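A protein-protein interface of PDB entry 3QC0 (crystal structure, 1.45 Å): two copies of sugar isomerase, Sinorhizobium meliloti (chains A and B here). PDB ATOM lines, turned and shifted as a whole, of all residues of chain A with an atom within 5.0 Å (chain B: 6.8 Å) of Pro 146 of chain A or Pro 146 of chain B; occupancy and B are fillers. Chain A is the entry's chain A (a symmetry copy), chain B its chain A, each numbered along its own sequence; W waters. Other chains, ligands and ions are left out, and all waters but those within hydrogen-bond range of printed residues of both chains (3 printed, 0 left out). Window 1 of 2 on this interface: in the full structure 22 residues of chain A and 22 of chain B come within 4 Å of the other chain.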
ATOM      1  N   LEU A 144       1.997  15.321  -3.938  1.00  0.00           N
ATOM      2  CA  LEU A 144       2.996  15.809  -4.867  1.00  0.00           C
ATOM      3  C   LEU A 144       2.741  17.288  -5.123  1.00  0.00           C
ATOM      4  O   LEU A 144       1.618  17.779  -5.029  1.00  0.00           O
ATOM      5  CB  LEU A 144       2.995  15.054  -6.196  1.00  0.00           C
ATOM      6  CG  LEU A 144       4.218  14.144  -6.423  1.00  0.00           C
ATOM      7  CD1 LEU A 144       4.284  12.966  -5.425  1.00  0.00           C
ATOM      8  CD2 LEU A 144       4.265  13.718  -7.889  1.00  0.00           C
ATOM      9  N   HIS A 145       3.824  17.987  -5.463  1.00  0.00           N
ATOM     10  CA  HIS A 145       3.732  19.389  -5.745  1.00  0.00           C
ATOM     11  C   HIS A 145       2.593  19.615  -6.739  1.00  0.00           C
ATOM     12  O   HIS A 145       2.471  18.888  -7.717  1.00  0.00           O
ATOM     13  CB  HIS A 145       5.017  19.913  -6.361  1.00  0.00           C
ATOM     14  CG  HIS A 145       5.140  21.386  -6.270  1.00  0.00           C
ATOM     15  ND1 HIS A 145       4.443  22.243  -7.106  1.00  0.00           N
ATOM     16  CD2 HIS A 145       5.889  22.161  -5.444  1.00  0.00           C
ATOM     17  CE1 HIS A 145       4.782  23.497  -6.794  1.00  0.00           C
ATOM     18  NE2 HIS A 145       5.608  23.476  -5.757  1.00  0.00           N
ATOM     19  N   PRO A 146       1.825  20.689  -6.528  1.00  0.00           N
ATOM     20  CA  PRO A 146       0.750  20.996  -7.459  1.00  0.00           C
ATOM     21  C   PRO A 146       1.132  21.078  -8.937  1.00  0.00           C
ATOM     22  O   PRO A 146       0.279  20.849  -9.784  1.00  0.00           O
ATOM     23  CB  PRO A 146       0.214  22.348  -6.939  1.00  0.00           C
ATOM     24  CG  PRO A 146       0.359  22.188  -5.433  1.00  0.00           C
ATOM     25  CD  PRO A 146       1.667  21.401  -5.248  1.00  0.00           C
ATOM     26  N   MET A 147       2.387  21.396  -9.262  1.00  0.00           N
ATOM     27  CA  MET A 147       2.794  21.442 -10.659  1.00  0.00           C
ATOM     28  C   MET A 147       2.722  20.100 -11.357  1.00  0.00           C
ATOM     29  O   MET A 147       2.715  20.069 -12.587  1.00  0.00           O
ATOM     30  CB  MET A 147       4.184  22.069 -10.860  1.00  0.00           C
ATOM     31  CG  MET A 147       5.285  21.306 -10.291  1.00  0.00           C
ATOM     32  SD  MET A 147       6.940  22.486 -10.440  1.00  0.00           S
ATOM     33  CE  MET A 147       7.907  21.538  -9.105  1.00  0.00           C
ATOM     34  N   TYR A 148       2.627  19.008 -10.563  1.00  0.00           N
ATOM     35  CA  TYR A 148       2.511  17.663 -11.092  1.00  0.00           C
ATOM     36  C   TYR A 148       1.076  17.154 -11.245  1.00  0.00           C
ATOM     37  O   TYR A 148       0.849  15.993 -11.635  1.00  0.00           O
ATOM     38  CB  TYR A 148       3.272  16.701 -10.160  1.00  0.00           C
ATOM     39  CG  TYR A 148       4.747  17.089  -9.994  1.00  0.00           C
ATOM     40  CD1 TYR A 148       5.567  17.313 -11.102  1.00  0.00           C
ATOM     41  CD2 TYR A 148       5.322  17.222  -8.752  1.00  0.00           C
ATOM     42  CE1 TYR A 148       6.907  17.672 -10.952  1.00  0.00           C
ATOM     43  CE2 TYR A 148       6.648  17.562  -8.593  1.00  0.00           C
ATOM     44  CZ  TYR A 148       7.446  17.825  -9.688  1.00  0.00           C
ATOM     45  OH  TYR A 148       8.800  18.131  -9.495  1.00  0.00           O
ATOM     46  N   ALA A 149       0.085  17.985 -10.913  1.00  0.00           N
ATOM     47  CA  ALA A 149      -1.305  17.556 -10.814  1.00  0.00           C
ATOM     48  C   ALA A 149      -1.857  16.898 -12.056  1.00  0.00           C
ATOM     49  O   ALA A 149      -2.664  15.984 -11.965  1.00  0.00           O
ATOM     50  CB  ALA A 149      -2.229  18.731 -10.361  1.00  0.00           C
ATOM     51  N   ASN A 156      -2.390  16.455  -4.197  1.00  0.00           N
ATOM     52  CA  ASN A 156      -1.522  17.619  -4.227  1.00  0.00           C
ATOM     53  C   ASN A 156      -1.384  18.440  -2.966  1.00  0.00           C
ATOM     54  O   ASN A 156      -0.661  19.443  -2.980  1.00  0.00           O
ATOM     55  CB  ASN A 156      -1.979  18.526  -5.366  1.00  0.00           C
ATOM     56  CG  ASN A 156      -1.920  17.811  -6.688  1.00  0.00           C
ATOM     57  OD1 ASN A 156      -2.954  17.494  -7.280  1.00  0.00           O
ATOM     58  ND2 ASN A 156      -0.692  17.468  -7.124  1.00  0.00           N
ATOM     59  N   HIS A 180       7.411  18.821  -2.109  1.00  0.00           N
ATOM     60  CA  HIS A 180       6.034  18.829  -2.555  1.00  0.00           C
ATOM     61  C   HIS A 180       5.128  19.680  -1.676  1.00  0.00           C
ATOM     62  O   HIS A 180       4.039  20.087  -2.135  1.00  0.00           O
ATOM     63  CB  HIS A 180       5.493  17.395  -2.571  1.00  0.00           C
ATOM     64  CG  HIS A 180       6.232  16.503  -3.508  1.00  0.00           C
ATOM     65  ND1 HIS A 180       6.578  16.908  -4.781  1.00  0.00           N
ATOM     66  CD2 HIS A 180       6.679  15.225  -3.372  1.00  0.00           C
ATOM     67  CE1 HIS A 180       7.243  15.924  -5.374  1.00  0.00           C
ATOM     68  NE2 HIS A 180       7.309  14.896  -4.545  1.00  0.00           N
ATOM     69  N   TRP A 183       5.534  24.795   0.607  1.00  0.00           N
ATOM     70  CA  TRP A 183       4.813  26.027   0.260  1.00  0.00           C
ATOM     71  C   TRP A 183       3.434  26.122   0.873  1.00  0.00           C
ATOM     72  O   TRP A 183       2.804  27.165   0.860  1.00  0.00           O
ATOM     73  CB  TRP A 183       4.711  26.106  -1.318  1.00  0.00           C
ATOM     74  CG  TRP A 183       3.912  24.961  -1.771  1.00  0.00           C
ATOM     75  CD1 TRP A 183       4.398  23.714  -2.088  1.00  0.00           C
ATOM     76  CD2 TRP A 183       2.487  24.834  -1.776  1.00  0.00           C
ATOM     77  NE1 TRP A 183       3.378  22.849  -2.306  1.00  0.00           N
ATOM     78  CE2 TRP A 183       2.192  23.491  -2.102  1.00  0.00           C
ATOM     79  CE3 TRP A 183       1.415  25.734  -1.567  1.00  0.00           C
ATOM     80  CZ2 TRP A 183       0.900  23.013  -2.204  1.00  0.00           C
ATOM     81  CZ3 TRP A 183       0.135  25.249  -1.661  1.00  0.00           C
ATOM     82  CH2 TRP A 183      -0.116  23.905  -1.970  1.00  0.00           C
ATOM     83  N   LEU B 144      -1.255  32.774  -6.537  1.00  0.00           N
ATOM     84  CA  LEU B 144      -0.404  32.330  -7.623  1.00  0.00           C
ATOM     85  C   LEU B 144      -0.095  30.853  -7.426  1.00  0.00           C
ATOM     86  O   LEU B 144      -0.082  30.335  -6.311  1.00  0.00           O
ATOM     87  CB  LEU B 144       0.903  33.117  -7.718  1.00  0.00           C
ATOM     88  CG  LEU B 144       1.004  34.059  -8.933  1.00  0.00           C
ATOM     89  CD1 LEU B 144      -0.022  35.214  -8.885  1.00  0.00           C
ATOM     90  CD2 LEU B 144       2.451  34.520  -9.095  1.00  0.00           C
ATOM     91  N   HIS B 145       0.166  30.186  -8.551  1.00  0.00           N
ATOM     92  CA  HIS B 145       0.486  28.790  -8.516  1.00  0.00           C
ATOM     93  C   HIS B 145       1.578  28.562  -7.473  1.00  0.00           C
ATOM     94  O   HIS B 145       2.547  29.310  -7.417  1.00  0.00           O
ATOM     95  CB  HIS B 145       1.000  28.309  -9.861  1.00  0.00           C
ATOM     96  CG  HIS B 145       0.931  26.837 -10.012  1.00  0.00           C
ATOM     97  ND1 HIS B 145       1.843  25.986  -9.410  1.00  0.00           N
ATOM     98  CD2 HIS B 145       0.062  26.059 -10.706  1.00  0.00           C
ATOM     99  CE1 HIS B 145       1.531  24.732  -9.751  1.00  0.00           C
ATOM    100  NE2 HIS B 145       0.426  24.746 -10.485  1.00  0.00           N
ATOM    101  N   PRO B 146       1.458  27.467  -6.715  1.00  0.00           N
ATOM    102  CA  PRO B 146       2.484  27.159  -5.732  1.00  0.00           C
ATOM    103  C   PRO B 146       3.925  27.120  -6.240  1.00  0.00           C
ATOM    104  O   PRO B 146       4.837  27.352  -5.457  1.00  0.00           O
ATOM    105  CB  PRO B 146       2.042  25.784  -5.186  1.00  0.00           C
ATOM    106  CG  PRO B 146       0.526  25.910  -5.198  1.00  0.00           C
ATOM    107  CD  PRO B 146       0.212  26.722  -6.466  1.00  0.00           C
ATOM    108  N   MET B 147       4.148  26.838  -7.525  1.00  0.00           N
ATOM    109  CA  MET B 147       5.505  26.835  -8.051  1.00  0.00           C
ATOM    110  C   MET B 147       6.178  28.191  -8.007  1.00  0.00           C
ATOM    111  O   MET B 147       7.403  28.251  -8.105  1.00  0.00           O
ATOM    112  CB  MET B 147       5.600  26.244  -9.468  1.00  0.00           C
ATOM    113  CG  MET B 147       4.922  27.017 -10.497  1.00  0.00           C
ATOM    114  SD  MET B 147       4.954  25.877 -12.188  1.00  0.00           S
ATOM    115  CE  MET B 147       3.521  26.814 -13.014  1.00  0.00           C
ATOM    116  N   TYR B 148       5.371  29.261  -7.819  1.00  0.00           N
ATOM    117  CA  TYR B 148       5.878  30.616  -7.715  1.00  0.00           C
ATOM    118  C   TYR B 148       6.142  31.097  -6.288  1.00  0.00           C
ATOM    119  O   TYR B 148       6.525  32.261  -6.067  1.00  0.00           O
ATOM    120  CB  TYR B 148       4.863  31.572  -8.372  1.00  0.00           C
ATOM    121  CG  TYR B 148       4.580  31.213  -9.835  1.00  0.00           C
ATOM    122  CD1 TYR B 148       5.617  31.033 -10.752  1.00  0.00           C
ATOM    123  CD2 TYR B 148       3.296  31.063 -10.306  1.00  0.00           C
ATOM    124  CE1 TYR B 148       5.361  30.701 -12.082  1.00  0.00           C
ATOM    125  CE2 TYR B 148       3.031  30.748 -11.621  1.00  0.00           C
ATOM    126  CZ  TYR B 148       4.059  30.529 -12.515  1.00  0.00           C
ATOM    127  OH  TYR B 148       3.757  30.248 -13.855  1.00  0.00           O
ATOM    128  N   ALA B 149       5.916  30.237  -5.292  1.00  0.00           N
ATOM    129  CA  ALA B 149       5.927  30.633  -3.889  1.00  0.00           C
ATOM    130  C   ALA B 149       7.197  31.308  -3.429  1.00  0.00           C
ATOM    131  O   ALA B 149       7.155  32.201  -2.596  1.00  0.00           O
ATOM    132  CB  ALA B 149       5.581  29.427  -2.958  1.00  0.00           C
ATOM    133  N   ALA B 150       8.353  30.792  -3.866  1.00  0.00           N
ATOM    134  CA  ALA B 150       9.619  31.256  -3.298  1.00  0.00           C
ATOM    135  C   ALA B 150      10.048  32.613  -3.794  1.00  0.00           C
ATOM    136  O   ALA B 150      10.697  33.340  -3.068  1.00  0.00           O
ATOM    137  CB  ALA B 150      10.761  30.244  -3.562  1.00  0.00           C
ATOM    138  N   ALA B 153       5.402  35.005  -5.589  1.00  0.00           N
ATOM    139  CA  ALA B 153       4.198  35.265  -4.780  1.00  0.00           C
ATOM    140  C   ALA B 153       3.994  34.183  -3.794  1.00  0.00           C
ATOM    141  O   ALA B 153       3.781  33.047  -4.206  1.00  0.00           O
ATOM    142  CB  ALA B 153       2.908  35.405  -5.653  1.00  0.00           C
ATOM    143  N   VAL B 155       1.404  34.071  -1.749  1.00  0.00           N
ATOM    144  CA  VAL B 155      -0.045  33.814  -1.551  1.00  0.00           C
ATOM    145  C   VAL B 155      -0.361  32.802  -2.650  1.00  0.00           C
ATOM    146  O   VAL B 155      -0.273  33.112  -3.835  1.00  0.00           O
ATOM    147  CB  VAL B 155      -0.929  35.038  -1.670  1.00  0.00           C
ATOM    148  CG1 VAL B 155      -2.440  34.619  -1.565  1.00  0.00           C
ATOM    149  CG2 VAL B 155      -0.547  36.081  -0.590  1.00  0.00           C
ATOM    150  N   ASN B 156      -0.595  31.551  -2.216  1.00  0.00           N
ATOM    151  CA  ASN B 156      -0.614  30.406  -3.112  1.00  0.00           C
ATOM    152  C   ASN B 156      -1.864  29.559  -3.161  1.00  0.00           C
ATOM    153  O   ASN B 156      -1.890  28.573  -3.906  1.00  0.00           O
ATOM    154  CB  ASN B 156       0.579  29.517  -2.776  1.00  0.00           C
ATOM    155  CG  ASN B 156       1.876  30.265  -2.929  1.00  0.00           C
ATOM    156  OD1 ASN B 156       2.548  30.574  -1.942  1.00  0.00           O
ATOM    157  ND2 ASN B 156       2.197  30.645  -4.182  1.00  0.00           N
ATOM    158  N   THR B 157      -2.888  29.888  -2.362  1.00  0.00           N
ATOM    159  CA  THR B 157      -4.179  29.199  -2.461  1.00  0.00           C
ATOM    160  C   THR B 157      -5.295  30.236  -2.375  1.00  0.00           C
ATOM    161  O   THR B 157      -5.143  31.299  -1.735  1.00  0.00           O
ATOM    162  CB  THR B 157      -4.386  28.125  -1.380  1.00  0.00           C
ATOM    163  OG1 THR B 157      -4.629  28.758  -0.113  1.00  0.00           O
ATOM    164  CG2 THR B 157      -3.189  27.093  -1.381  1.00  0.00           C
ATOM    165  N   TYR B 179      -5.013  29.292 -14.120  1.00  0.00           N
ATOM    166  CA  TYR B 179      -3.670  28.709 -14.163  1.00  0.00           C
ATOM    167  C   TYR B 179      -3.152  28.435 -12.765  1.00  0.00           C
ATOM    168  O   TYR B 179      -2.490  27.466 -12.492  1.00  0.00           O
ATOM    169  CB  TYR B 179      -2.668  29.624 -14.887  1.00  0.00           C
ATOM    170  CG  TYR B 179      -1.493  28.886 -15.472  1.00  0.00           C
ATOM    171  CD1 TYR B 179      -1.663  28.041 -16.566  1.00  0.00           C
ATOM    172  CD2 TYR B 179      -0.206  29.022 -14.949  1.00  0.00           C
ATOM    173  CE1 TYR B 179      -0.596  27.337 -17.106  1.00  0.00           C
ATOM    174  CE2 TYR B 179       0.881  28.344 -15.505  1.00  0.00           C
ATOM    175  CZ  TYR B 179       0.674  27.496 -16.590  1.00  0.00           C
ATOM    176  OH  TYR B 179       1.739  26.830 -17.168  1.00  0.00           O
ATOM    177  N   HIS B 180      -3.465  29.351 -11.857  1.00  0.00           N
ATOM    178  CA  HIS B 180      -2.903  29.324 -10.524  1.00  0.00           C
ATOM    179  C   HIS B 180      -3.681  28.432  -9.567  1.00  0.00           C
ATOM    180  O   HIS B 180      -3.121  28.012  -8.531  1.00  0.00           O
ATOM    181  CB  HIS B 180      -2.871  30.745  -9.952  1.00  0.00           C
ATOM    182  CG  HIS B 180      -2.021  31.675 -10.746  1.00  0.00           C
ATOM    183  ND1 HIS B 180      -0.774  31.309 -11.210  1.00  0.00           N
ATOM    184  CD2 HIS B 180      -2.223  32.959 -11.150  1.00  0.00           C
ATOM    185  CE1 HIS B 180      -0.262  32.321 -11.899  1.00  0.00           C
ATOM    186  NE2 HIS B 180      -1.116  33.330 -11.869  1.00  0.00           N
ATOM    187  N   VAL B 181      -4.979  28.218  -9.855  1.00  0.00           N
ATOM    188  CA  VAL B 181      -5.871  27.568  -8.878  1.00  0.00           C
ATOM    189  C   VAL B 181      -6.538  26.262  -9.325  1.00  0.00           C
ATOM    190  O   VAL B 181      -7.167  25.614  -8.482  1.00  0.00           O
ATOM    191  CB  VAL B 181      -7.024  28.564  -8.420  1.00  0.00           C
ATOM    192  CG1 VAL B 181      -6.475  29.900  -7.955  1.00  0.00           C
ATOM    193  CG2 VAL B 181      -8.091  28.777  -9.549  1.00  0.00           C
ATOM    194  N   TRP B 182      -6.452  25.897 -10.609  1.00  0.00           N
ATOM    195  CA  TRP B 182      -7.280  24.812 -11.158  1.00  0.00           C
ATOM    196  C   TRP B 182      -7.093  23.490 -10.392  1.00  0.00           C
ATOM    197  O   TRP B 182      -8.018  22.694 -10.302  1.00  0.00           O
ATOM    198  CB  TRP B 182      -6.997  24.569 -12.637  1.00  0.00           C
ATOM    199  CG  TRP B 182      -5.697  23.927 -12.895  1.00  0.00           C
ATOM    200  CD1 TRP B 182      -4.488  24.516 -12.970  1.00  0.00           C
ATOM    201  CD2 TRP B 182      -5.469  22.511 -13.020  1.00  0.00           C
ATOM    202  NE1 TRP B 182      -3.506  23.560 -13.161  1.00  0.00           N
ATOM    203  CE2 TRP B 182      -4.098  22.321 -13.206  1.00  0.00           C
ATOM    204  CE3 TRP B 182      -6.312  21.427 -13.044  1.00  0.00           C
ATOM    205  CZ2 TRP B 182      -3.529  21.043 -13.384  1.00  0.00           C
ATOM    206  CZ3 TRP B 182      -5.779  20.170 -13.187  1.00  0.00           C
ATOM    207  CH2 TRP B 182      -4.378  19.976 -13.366  1.00  0.00           C
ATOM    208  N   TRP B 183      -5.878  23.274  -9.899  1.00  0.00           N
ATOM    209  CA  TRP B 183      -5.443  22.035  -9.240  1.00  0.00           C
ATOM    210  C   TRP B 183      -5.933  21.896  -7.816  1.00  0.00           C
ATOM    211  O   TRP B 183      -5.843  20.839  -7.214  1.00  0.00           O
ATOM    212  CB  TRP B 183      -3.860  21.992  -9.275  1.00  0.00           C
ATOM    213  CG  TRP B 183      -3.366  23.129  -8.490  1.00  0.00           C
ATOM    214  CD1 TRP B 183      -3.119  24.394  -8.972  1.00  0.00           C
ATOM    215  CD2 TRP B 183      -3.242  23.225  -7.068  1.00  0.00           C
ATOM    216  NE1 TRP B 183      -2.833  25.241  -7.954  1.00  0.00           N
ATOM    217  CE2 TRP B 183      -2.920  24.568  -6.770  1.00  0.00           C
ATOM    218  CE3 TRP B 183      -3.337  22.297  -6.004  1.00  0.00           C
ATOM    219  CZ2 TRP B 183      -2.718  25.020  -5.480  1.00  0.00           C
ATOM    220  CZ3 TRP B 183      -3.145  22.756  -4.726  1.00  0.00           C
ATOM    221  CH2 TRP B 183      -2.845  24.101  -4.469  1.00  0.00           C
ATOM    222  N   ASP B 184      -6.427  22.986  -7.217  1.00  0.00           N
ATOM    223  CA  ASP B 184      -6.661  23.002  -5.782  1.00  0.00           C
ATOM    224  C   ASP B 184      -7.812  22.058  -5.421  1.00  0.00           C
ATOM    225  O   ASP B 184      -8.927  22.229  -5.894  1.00  0.00           O
ATOM    226  CB  ASP B 184      -6.973  24.437  -5.335  1.00  0.00           C
ATOM    227  CG  ASP B 184      -7.047  24.605  -3.819  1.00  0.00           C
ATOM    228  OD1 ASP B 184      -7.392  23.669  -3.090  1.00  0.00           O
ATOM    229  OD2 ASP B 184      -6.738  25.725  -3.349  1.00  0.00           O
ATOM    230  N   TRP B 208      -3.807  24.774 -18.814  1.00  0.00           N
ATOM    231  CA  TRP B 208      -2.665  24.030 -18.317  1.00  0.00           C
ATOM    232  C   TRP B 208      -2.343  22.903 -19.277  1.00  0.00           C
ATOM    233  O   TRP B 208      -3.140  21.987 -19.442  1.00  0.00           O
ATOM    234  CB  TRP B 208      -2.956  23.488 -16.893  1.00  0.00           C
ATOM    235  CG  TRP B 208      -1.737  22.805 -16.320  1.00  0.00           C
ATOM    236  CD1 TRP B 208      -1.342  21.501 -16.539  1.00  0.00           C
ATOM    237  CD2 TRP B 208      -0.723  23.381 -15.489  1.00  0.00           C
ATOM    238  NE1 TRP B 208      -0.186  21.242 -15.858  1.00  0.00           N
ATOM    239  CE2 TRP B 208       0.220  22.378 -15.213  1.00  0.00           C
ATOM    240  CE3 TRP B 208      -0.560  24.604 -14.895  1.00  0.00           C
ATOM    241  CZ2 TRP B 208       1.331  22.612 -14.428  1.00  0.00           C
ATOM    242  CZ3 TRP B 208       0.547  24.849 -14.136  1.00  0.00           C
ATOM    243  CH2 TRP B 208       1.469  23.847 -13.877  1.00  0.00           C
HETATM  244  O   HOH W   1       0.993  18.743 -14.226  1.00  0.00           O
HETATM  245  O   HOH W   2      -0.741  22.492 -11.767  1.00  0.00           O
HETATM  246  O   HOH W   3       6.937  25.734  -4.650  1.00  0.00           O
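Of the 18 printed residues of chain B, 8 touch a printed residue of chain A. Hydrophobic or aromatic side chains of chain B within 4 Å of the printed part of chain A: His 145, Pro 146, Met 147, Ala 149, Trp 182, Trp 183 and Trp 208. Of the 9 printed residues of chain A, 5 touch a printed residue of chain B. Hydrophobic or aromatic side chains of chain A within 4 Å of the printed part of chain B: His 145, Pro 146, Met 147, Ala 149 and Trp 183. Among the printed residues, 13 pairs touch across the chains. Among the printed residues, no Asp or Glu carboxylate lies within 4 Å of a Lys or Arg side-chain nitrogen of the other chain.
Printed residues of chain A within 4 Å of Pro 146 of chain B: His 145, Pro 146 and Trp 183. Printed residues of chain A within 4 Å of Trp 183 of chain B: Pro 146, Ala 149 and Trp 183. Of the printed residues of chain A, Ala 149 of chain B touches Trp 183. Printed residues of chain A within 4 Å of Trp 208 of chain B: Met 147 (3.4 Å). Of the printed residues of chain A, Met 147 of chain B touches His 145. The nearest residue of chain B that does not touch Pro 146 of chain A is Trp 208 of chain B (5.1 Å). The nearest printed residue of chain A that does not touch Pro 146 of chain B is Met 147 of chain A (6.0 Å). The nearest printed residue of chain B that does not touch His 145 of chain A is His 145 of chain B (4.6 Å).
N of His 145 of chain A sits at hydrogen-bond distance from ND1 of His 180 of chain A, 3.0 Å away. A ring nitrogen (ND1) of His 145 of chain B sits close to the backbone NH of Met 147 of chain B, at 3.1 Å. A ring nitrogen (ND1) of His 145 of chain A sits close to the backbone NH (N) of Met 147 of chain A (3.1 Å). The backbone carbonyl oxygen (O) of His 180 of chain B is in hydrogen-bond range of the indole nitrogen (NE1) of Trp 183 of chain B (2.8 Å). O of His 180 of chain A lies within hydrogen-bond range of NE1 of Trp 183 of chain A, at 2.8 Å. ND1 of His 180 of chain B lies within hydrogen-bond range of N of His 145 of chain B (3.0 Å).
Water W1 lies within hydrogen-bond range of O of Met 147 of chain A and NE1 of Trp 208 of chain B. Water W3 lies within hydrogen-bond range of O of Pro 146 of chain B and NE2 of His 145 of chain A. Water W2 lies within hydrogen-bond range of O of Pro 146 of chain A (2.8 Å), NE2 of His 145 of chain B (2.8 Å) and NE1 of Trp 182 of chain B (3.3 Å).
Among the printed residues, merely in contact across the chains: His 145 of chain A with Pro 146 of chain B (3.8 Å), His 145 of chain A with Met 147 of chain B (3.5 Å), Pro 146 of chain A with His 145 of chain B (3.8 Å), Pro 146 of chain A with Pro 146 of chain B (3.7 Å), Pro 146 of chain A with Trp 183 of chain B (3.6 Å), Met 147 of chain A with His 145 of chain B (3.5 Å), Met 147 of chain A with Trp 208 of chain B (3.4 Å), Ala 149 of chain A with Trp 182 of chain B (3.9 Å), Ala 149 of chain A with Trp 183 of chain B (3.8 Å), Trp 183 of chain A with Pro 146 of chain B (3.6 Å), Trp 183 of chain A with Ala 149 of chain B (3.8 Å), Trp 183 of chain A with Thr 157 of chain B (3.8 Å) and Trp 183 of chain A with Trp 183 of chain B (3.7 Å).
His 145 of chain A touches Pro 146 of chain B, and with the chains exchanged Pro 146 of chain A touches His 145 of chain B. Pro 146 of chain B touches its own counterpart, Pro 146 of chain A. Pro 146 of chain A touches Trp 183 of chain B, and with the chains exchanged Trp 183 of chain A touches Pro 146 of chain B. Trp 183 of chain B touches its own counterpart, Trp 183 of chain A. Positions printed for both chains: 144, 145, 146, 147, 148, 149, 156, 180 and 183. Of the 13 pairs that touch across the chains among the printed residues, 10 have their exchanged pair printed and touching as well.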
